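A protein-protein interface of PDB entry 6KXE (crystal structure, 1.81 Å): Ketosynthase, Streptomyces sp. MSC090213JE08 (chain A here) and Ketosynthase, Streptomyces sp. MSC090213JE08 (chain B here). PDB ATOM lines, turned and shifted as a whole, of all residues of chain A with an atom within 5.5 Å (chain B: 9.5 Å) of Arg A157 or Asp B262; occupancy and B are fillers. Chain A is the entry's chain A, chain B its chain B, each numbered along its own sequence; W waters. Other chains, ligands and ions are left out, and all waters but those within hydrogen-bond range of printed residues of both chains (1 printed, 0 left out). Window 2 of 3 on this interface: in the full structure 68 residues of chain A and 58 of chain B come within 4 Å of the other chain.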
ATOM      1  N   HIS A  69     -13.244 -13.283 -16.334  1.00  0.00           N
ATOM      2  CA  HIS A  69     -13.972 -12.021 -16.081  1.00  0.00           C
ATOM      3  C   HIS A  69     -13.036 -10.816 -16.112  1.00  0.00           C
ATOM      4  O   HIS A  69     -13.458  -9.758 -16.605  1.00  0.00           O
ATOM      5  CB  HIS A  69     -14.674 -12.118 -14.732  1.00  0.00           C
ATOM      6  CG  HIS A  69     -15.697 -13.195 -14.692  1.00  0.00           C
ATOM      7  ND1 HIS A  69     -15.848 -14.035 -13.625  1.00  0.00           N
ATOM      8  CD2 HIS A  69     -16.652 -13.541 -15.585  1.00  0.00           C
ATOM      9  CE1 HIS A  69     -16.874 -14.837 -13.839  1.00  0.00           C
ATOM     10  NE2 HIS A  69     -17.325 -14.605 -15.062  1.00  0.00           N
ATOM     11  N   GLU A  97     -18.471 -20.111  -8.202  1.00  0.00           N
ATOM     12  CA  GLU A  97     -18.718 -18.657  -8.007  1.00  0.00           C
ATOM     13  C   GLU A  97     -20.024 -18.427  -7.224  1.00  0.00           C
ATOM     14  O   GLU A  97     -20.030 -17.541  -6.364  1.00  0.00           O
ATOM     15  CB  GLU A  97     -18.740 -17.928  -9.345  1.00  0.00           C
ATOM     16  CG  GLU A  97     -17.361 -17.817  -9.954  1.00  0.00           C
ATOM     17  CD  GLU A  97     -17.388 -17.288 -11.376  1.00  0.00           C
ATOM     18  OE1 GLU A  97     -18.362 -16.564 -11.720  1.00  0.00           O
ATOM     19  OE2 GLU A  97     -16.447 -17.616 -12.134  1.00  0.00           O
ATOM     20  N   GLY A 101     -20.087 -16.289  -3.645  1.00  0.00           N
ATOM     21  CA  GLY A 101     -20.672 -14.960  -3.898  1.00  0.00           C
ATOM     22  C   GLY A 101     -20.998 -14.206  -2.637  1.00  0.00           C
ATOM     23  O   GLY A 101     -20.464 -13.103  -2.453  1.00  0.00           O
ATOM     24  N   ILE A 152      -8.571 -11.088  -7.495  1.00  0.00           N
ATOM     25  CA  ILE A 152      -9.162 -12.421  -7.224  1.00  0.00           C
ATOM     26  C   ILE A 152     -10.648 -12.214  -6.873  1.00  0.00           C
ATOM     27  O   ILE A 152     -11.513 -12.986  -7.383  1.00  0.00           O
ATOM     28  CB  ILE A 152      -8.392 -13.166  -6.123  1.00  0.00           C
ATOM     29  CG1 ILE A 152      -6.960 -13.482  -6.545  1.00  0.00           C
ATOM     30  CG2 ILE A 152      -9.149 -14.422  -5.668  1.00  0.00           C
ATOM     31  CD1 ILE A 152      -6.099 -13.954  -5.392  1.00  0.00           C
ATOM     32  N   ALA A 153     -10.959 -11.285  -5.959  1.00  0.00           N
ATOM     33  CA  ALA A 153     -12.369 -10.966  -5.594  1.00  0.00           C
ATOM     34  C   ALA A 153     -13.168 -10.600  -6.869  1.00  0.00           C
ATOM     35  O   ALA A 153     -14.332 -11.019  -7.010  1.00  0.00           O
ATOM     36  CB  ALA A 153     -12.434  -9.831  -4.586  1.00  0.00           C
ATOM     37  N   ARG A 154     -12.575  -9.814  -7.768  1.00  0.00           N
ATOM     38  CA  ARG A 154     -13.244  -9.438  -9.046  1.00  0.00           C
ATOM     39  C   ARG A 154     -13.446 -10.688  -9.897  1.00  0.00           C
ATOM     40  O   ARG A 154     -14.558 -10.846 -10.421  1.00  0.00           O
ATOM     41  CB  ARG A 154     -12.475  -8.392  -9.856  1.00  0.00           C
ATOM     42  CG  ARG A 154     -12.522  -7.009  -9.239  1.00  0.00           C
ATOM     43  CD  ARG A 154     -11.646  -6.011  -9.965  1.00  0.00           C
ATOM     44  NE  ARG A 154     -11.978  -5.987 -11.382  1.00  0.00           N
ATOM     45  CZ  ARG A 154     -11.162  -5.501 -12.318  1.00  0.00           C
ATOM     46  NH1 ARG A 154      -9.975  -5.034 -11.969  1.00  0.00           N
ATOM     47  NH2 ARG A 154     -11.524  -5.519 -13.586  1.00  0.00           N
ATOM     48  N   GLU A 155     -12.452 -11.549 -10.049  1.00  0.00           N
ATOM     49  CA  GLU A 155     -12.607 -12.740 -10.924  1.00  0.00           C
ATOM     50  C   GLU A 155     -13.673 -13.678 -10.366  1.00  0.00           C
ATOM     51  O   GLU A 155     -14.452 -14.227 -11.159  1.00  0.00           O
ATOM     52  CB  GLU A 155     -11.276 -13.458 -11.062  1.00  0.00           C
ATOM     53  CG  GLU A 155     -11.375 -14.736 -11.842  1.00  0.00           C
ATOM     54  CD  GLU A 155     -11.739 -14.565 -13.311  1.00  0.00           C
ATOM     55  OE1 GLU A 155     -11.685 -13.412 -13.860  1.00  0.00           O
ATOM     56  OE2 GLU A 155     -12.084 -15.588 -13.912  1.00  0.00           O
ATOM     57  N   LEU A 156     -13.696 -13.871  -9.056  1.00  0.00           N
ATOM     58  CA  LEU A 156     -14.619 -14.807  -8.393  1.00  0.00           C
ATOM     59  C   LEU A 156     -15.961 -14.163  -8.065  1.00  0.00           C
ATOM     60  O   LEU A 156     -16.804 -14.894  -7.583  1.00  0.00           O
ATOM     61  CB  LEU A 156     -13.924 -15.380  -7.159  1.00  0.00           C
ATOM     62  CG  LEU A 156     -12.655 -16.183  -7.447  1.00  0.00           C
ATOM     63  CD1 LEU A 156     -12.117 -16.822  -6.186  1.00  0.00           C
ATOM     64  CD2 LEU A 156     -12.878 -17.268  -8.485  1.00  0.00           C
ATOM     65  N   ARG A 157     -16.187 -12.891  -8.404  1.00  0.00           N
ATOM     66  CA  ARG A 157     -17.469 -12.188  -8.155  1.00  0.00           C
ATOM     67  C   ARG A 157     -17.789 -12.250  -6.653  1.00  0.00           C
ATOM     68  O   ARG A 157     -18.970 -12.490  -6.270  1.00  0.00           O
ATOM     69  CB  ARG A 157     -18.551 -12.762  -9.090  1.00  0.00           C
ATOM     70  CG  ARG A 157     -18.223 -12.584 -10.574  1.00  0.00           C
ATOM     71  CD  ARG A 157     -18.078 -11.138 -11.009  1.00  0.00           C
ATOM     72  NE  ARG A 157     -19.313 -10.422 -10.692  1.00  0.00           N
ATOM     73  CZ  ARG A 157     -19.543  -9.116 -10.821  1.00  0.00           C
ATOM     74  NH1 ARG A 157     -18.607  -8.308 -11.284  1.00  0.00           N
ATOM     75  NH2 ARG A 157     -20.734  -8.632 -10.477  1.00  0.00           N
ATOM     76  N   MET A 158     -16.784 -11.964  -5.821  1.00  0.00           N
ATOM     77  CA  MET A 158     -16.931 -11.958  -4.343  1.00  0.00           C
ATOM     78  C   MET A 158     -16.745 -10.539  -3.835  1.00  0.00           C
ATOM     79  O   MET A 158     -15.622 -10.122  -3.623  1.00  0.00           O
ATOM     80  CB  MET A 158     -15.882 -12.873  -3.721  1.00  0.00           C
ATOM     81  CG  MET A 158     -16.049 -14.307  -4.117  1.00  0.00           C
ATOM     82  SD  MET A 158     -14.718 -15.326  -3.536  1.00  0.00           S
ATOM     83  CE  MET A 158     -15.254 -15.420  -1.828  1.00  0.00           C
ATOM     84  N   PRO A 159     -17.808  -9.735  -3.638  1.00  0.00           N
ATOM     85  CA  PRO A 159     -17.648  -8.379  -3.097  1.00  0.00           C
ATOM     86  C   PRO A 159     -17.444  -8.275  -1.572  1.00  0.00           C
ATOM     87  O   PRO A 159     -16.846  -7.287  -1.088  1.00  0.00           O
ATOM     88  CB  PRO A 159     -18.988  -7.718  -3.444  1.00  0.00           C
ATOM     89  CG  PRO A 159     -19.978  -8.872  -3.402  1.00  0.00           C
ATOM     90  CD  PRO A 159     -19.213 -10.072  -3.918  1.00  0.00           C
ATOM     91  N   ARG B 258     -14.871  -4.333   1.792  1.00  0.00           N
ATOM     92  CA  ARG B 258     -15.496  -4.885   0.577  1.00  0.00           C
ATOM     93  C   ARG B 258     -14.521  -4.690  -0.557  1.00  0.00           C
ATOM     94  O   ARG B 258     -13.587  -3.892  -0.433  1.00  0.00           O
ATOM     95  CB  ARG B 258     -16.789  -4.136   0.244  1.00  0.00           C
ATOM     96  CG  ARG B 258     -18.015  -4.684   0.956  1.00  0.00           C
ATOM     97  CD  ARG B 258     -19.276  -3.938   0.560  1.00  0.00           C
ATOM     98  NE  ARG B 258     -19.978  -4.494  -0.592  1.00  0.00           N
ATOM     99  CZ  ARG B 258     -20.722  -5.596  -0.541  1.00  0.00           C
ATOM    100  NH1 ARG B 258     -20.837  -6.278   0.585  1.00  0.00           N
ATOM    101  NH2 ARG B 258     -21.339  -6.018  -1.628  1.00  0.00           N
ATOM    102  N   VAL B 259     -14.810  -5.345  -1.650  1.00  0.00           N
ATOM    103  CA  VAL B 259     -14.163  -5.033  -2.940  1.00  0.00           C
ATOM    104  C   VAL B 259     -15.264  -4.520  -3.858  1.00  0.00           C
ATOM    105  O   VAL B 259     -16.312  -5.152  -3.933  1.00  0.00           O
ATOM    106  CB  VAL B 259     -13.407  -6.232  -3.520  1.00  0.00           C
ATOM    107  CG1 VAL B 259     -12.849  -5.852  -4.872  1.00  0.00           C
ATOM    108  CG2 VAL B 259     -12.317  -6.686  -2.559  1.00  0.00           C
ATOM    109  N   ASP B 260     -15.014  -3.362  -4.455  1.00  0.00           N
ATOM    110  CA  ASP B 260     -15.911  -2.715  -5.432  1.00  0.00           C
ATOM    111  C   ASP B 260     -15.776  -3.442  -6.778  1.00  0.00           C
ATOM    112  O   ASP B 260     -15.128  -2.916  -7.680  1.00  0.00           O
ATOM    113  CB  ASP B 260     -15.539  -1.244  -5.553  1.00  0.00           C
ATOM    114  CG  ASP B 260     -16.480  -0.470  -6.453  1.00  0.00           C
ATOM    115  OD1 ASP B 260     -17.560  -1.022  -6.793  1.00  0.00           O
ATOM    116  OD2 ASP B 260     -16.129   0.680  -6.782  1.00  0.00           O
ATOM    117  N   ILE B 261     -16.404  -4.591  -6.933  1.00  0.00           N
ATOM    118  CA  ILE B 261     -16.263  -5.399  -8.180  1.00  0.00           C
ATOM    119  C   ILE B 261     -17.126  -4.839  -9.326  1.00  0.00           C
ATOM    120  O   ILE B 261     -16.844  -5.246 -10.452  1.00  0.00           O
ATOM    121  CB  ILE B 261     -16.586  -6.877  -7.924  1.00  0.00           C
ATOM    122  CG1 ILE B 261     -18.058  -7.071  -7.593  1.00  0.00           C
ATOM    123  CG2 ILE B 261     -15.668  -7.473  -6.866  1.00  0.00           C
ATOM    124  CD1 ILE B 261     -18.438  -8.508  -7.349  1.00  0.00           C
ATOM    125  N   ASP B 262     -18.127  -3.990  -9.074  1.00  0.00           N
ATOM    126  CA  ASP B 262     -19.057  -3.437 -10.115  1.00  0.00           C
ATOM    127  C   ASP B 262     -18.661  -1.999 -10.482  1.00  0.00           C
ATOM    128  O   ASP B 262     -19.456  -1.326 -11.103  1.00  0.00           O
ATOM    129  CB  ASP B 262     -20.506  -3.506  -9.636  1.00  0.00           C
ATOM    130  CG  ASP B 262     -20.990  -4.931  -9.395  1.00  0.00           C
ATOM    131  OD1 ASP B 262     -20.642  -5.808 -10.221  1.00  0.00           O
ATOM    132  OD2 ASP B 262     -21.652  -5.169  -8.347  1.00  0.00           O
ATOM    133  N   ASP B 263     -17.476  -1.535 -10.085  1.00  0.00           N
ATOM    134  CA  ASP B 263     -17.040  -0.124 -10.256  1.00  0.00           C
ATOM    135  C   ASP B 263     -18.214   0.805  -9.888  1.00  0.00           C
ATOM    136  O   ASP B 263     -18.576   1.697 -10.665  1.00  0.00           O
ATOM    137  CB  ASP B 263     -16.515   0.153 -11.669  1.00  0.00           C
ATOM    138  CG  ASP B 263     -15.733   1.460 -11.757  1.00  0.00           C
ATOM    139  OD1 ASP B 263     -15.132   1.860 -10.723  1.00  0.00           O
ATOM    140  OD2 ASP B 263     -15.730   2.075 -12.849  1.00  0.00           O
ATOM    141  N   ASP B 264     -18.797   0.598  -8.714  1.00  0.00           N
ATOM    142  CA  ASP B 264     -19.796   1.515  -8.134  1.00  0.00           C
ATOM    143  C   ASP B 264     -19.327   1.865  -6.728  1.00  0.00           C
ATOM    144  O   ASP B 264     -19.822   1.281  -5.765  1.00  0.00           O
ATOM    145  CB  ASP B 264     -21.173   0.866  -8.197  1.00  0.00           C
ATOM    146  CG  ASP B 264     -22.273   1.800  -7.726  1.00  0.00           C
ATOM    147  OD1 ASP B 264     -21.940   2.890  -7.149  1.00  0.00           O
ATOM    148  OD2 ASP B 264     -23.444   1.420  -7.905  1.00  0.00           O
ATOM    149  N   PRO B 265     -18.315   2.744  -6.563  1.00  0.00           N
ATOM    150  CA  PRO B 265     -17.745   2.970  -5.234  1.00  0.00           C
ATOM    151  C   PRO B 265     -18.726   3.521  -4.184  1.00  0.00           C
ATOM    152  O   PRO B 265     -18.607   3.148  -3.015  1.00  0.00           O
ATOM    153  CB  PRO B 265     -16.579   3.929  -5.485  1.00  0.00           C
ATOM    154  CG  PRO B 265     -16.796   4.489  -6.888  1.00  0.00           C
ATOM    155  CD  PRO B 265     -17.571   3.435  -7.630  1.00  0.00           C
ATOM    156  N   GLY B 266     -19.695   4.350  -4.604  1.00  0.00           N
ATOM    157  CA  GLY B 266     -20.775   4.833  -3.716  1.00  0.00           C
ATOM    158  C   GLY B 266     -21.560   3.701  -3.079  1.00  0.00           C
ATOM    159  O   GLY B 266     -21.798   3.724  -1.856  1.00  0.00           O
ATOM    160  N   ALA B 267     -22.017   2.738  -3.871  1.00  0.00           N
ATOM    161  CA  ALA B 267     -22.781   1.562  -3.372  1.00  0.00           C
ATOM    162  C   ALA B 267     -21.867   0.713  -2.470  1.00  0.00           C
ATOM    163  O   ALA B 267     -22.310   0.230  -1.396  1.00  0.00           O
ATOM    164  CB  ALA B 267     -23.326   0.755  -4.535  1.00  0.00           C
ATOM    165  N   ALA B 268     -20.606   0.545  -2.865  1.00  0.00           N
ATOM    166  CA  ALA B 268     -19.646  -0.300  -2.108  1.00  0.00           C
ATOM    167  C   ALA B 268     -19.392   0.351  -0.740  1.00  0.00           C
ATOM    168  O   ALA B 268     -19.470  -0.353   0.278  1.00  0.00           O
ATOM    169  CB  ALA B 268     -18.380  -0.499  -2.896  1.00  0.00           C
ATOM    170  N   GLY B 364      -9.700  -1.122  -5.750  1.00  0.00           N
ATOM    171  CA  GLY B 364     -11.049  -1.685  -5.567  1.00  0.00           C
ATOM    172  C   GLY B 364     -11.439  -1.884  -4.114  1.00  0.00           C
ATOM    173  O   GLY B 364     -12.628  -2.070  -3.844  1.00  0.00           O
ATOM    174  N   VAL B 366     -12.473  -1.277  -0.298  1.00  0.00           N
ATOM    175  CA  VAL B 366     -13.218  -0.256   0.481  1.00  0.00           C
ATOM    176  C   VAL B 366     -13.172  -0.707   1.925  1.00  0.00           C
ATOM    177  O   VAL B 366     -13.253  -1.955   2.181  1.00  0.00           O
ATOM    178  CB  VAL B 366     -14.660  -0.212  -0.053  1.00  0.00           C
ATOM    179  CG1 VAL B 366     -15.523   0.625   0.846  1.00  0.00           C
ATOM    180  CG2 VAL B 366     -14.676   0.280  -1.490  1.00  0.00           C
HETATM  181  O   HOH W   1     -14.806  -6.514 -11.778  1.00  0.00           O
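N of Val B259 sits at hydrogen-bond distance from O of Pro A159 (2.9 Å). The side-chain carboxylate (OD1) of Asp B262 is in salt-bridge range of the guanidinium group (NH2) of Arg A157 (2.8 Å).
The backbone carbonyl oxygen (O) of Ala A153 lies within hydrogen-bond range of the backbone NH (N) of Met A158 (2.9 Å). N of Val B366 sits at hydrogen-bond distance from O of Arg B258, at 2.8 Å.
CB of Ala A153 touches CG2 of Val B259 (3.7 Å). Ala A153 touches Ile B261 (O to CG2, 3.8 Å). CA of Arg A154 touches CG2 of Ile B261 (3.8 Å). Arg A157 touches Ile B261 (NH1 to O, 3.6 Å). Arg B258 touches Pro A159. Ile B261 touches Pro A159 (CD1 to CD, 3.8 Å).
Arg A157 touches just these residues of chain B: Ile B261 and Asp B262. Printed residues of chain A within 4 Å of Asp B262: Arg A157. Printed residues of chain B within 4 Å of Arg A154: Ile B261 (3.8 Å). Printed residues of chain A within 4 Å of Arg B258: Pro A159 (3.2 Å).
Printed residues of chain B that touch a printed residue of chain A: Arg B258, Val B259, Ile B261 and Asp B262. Hydrophobic or aromatic side chains of chain B within 4 Å of the printed part of chain A: Val B259 and Ile B261. Of the 11 printed residues of chain A, 4 touch a printed residue of chain B.
Water W1 lies within hydrogen-bond range of O of Ile B261 (2.7 Å) and NE of Arg A154 (2.9 Å).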
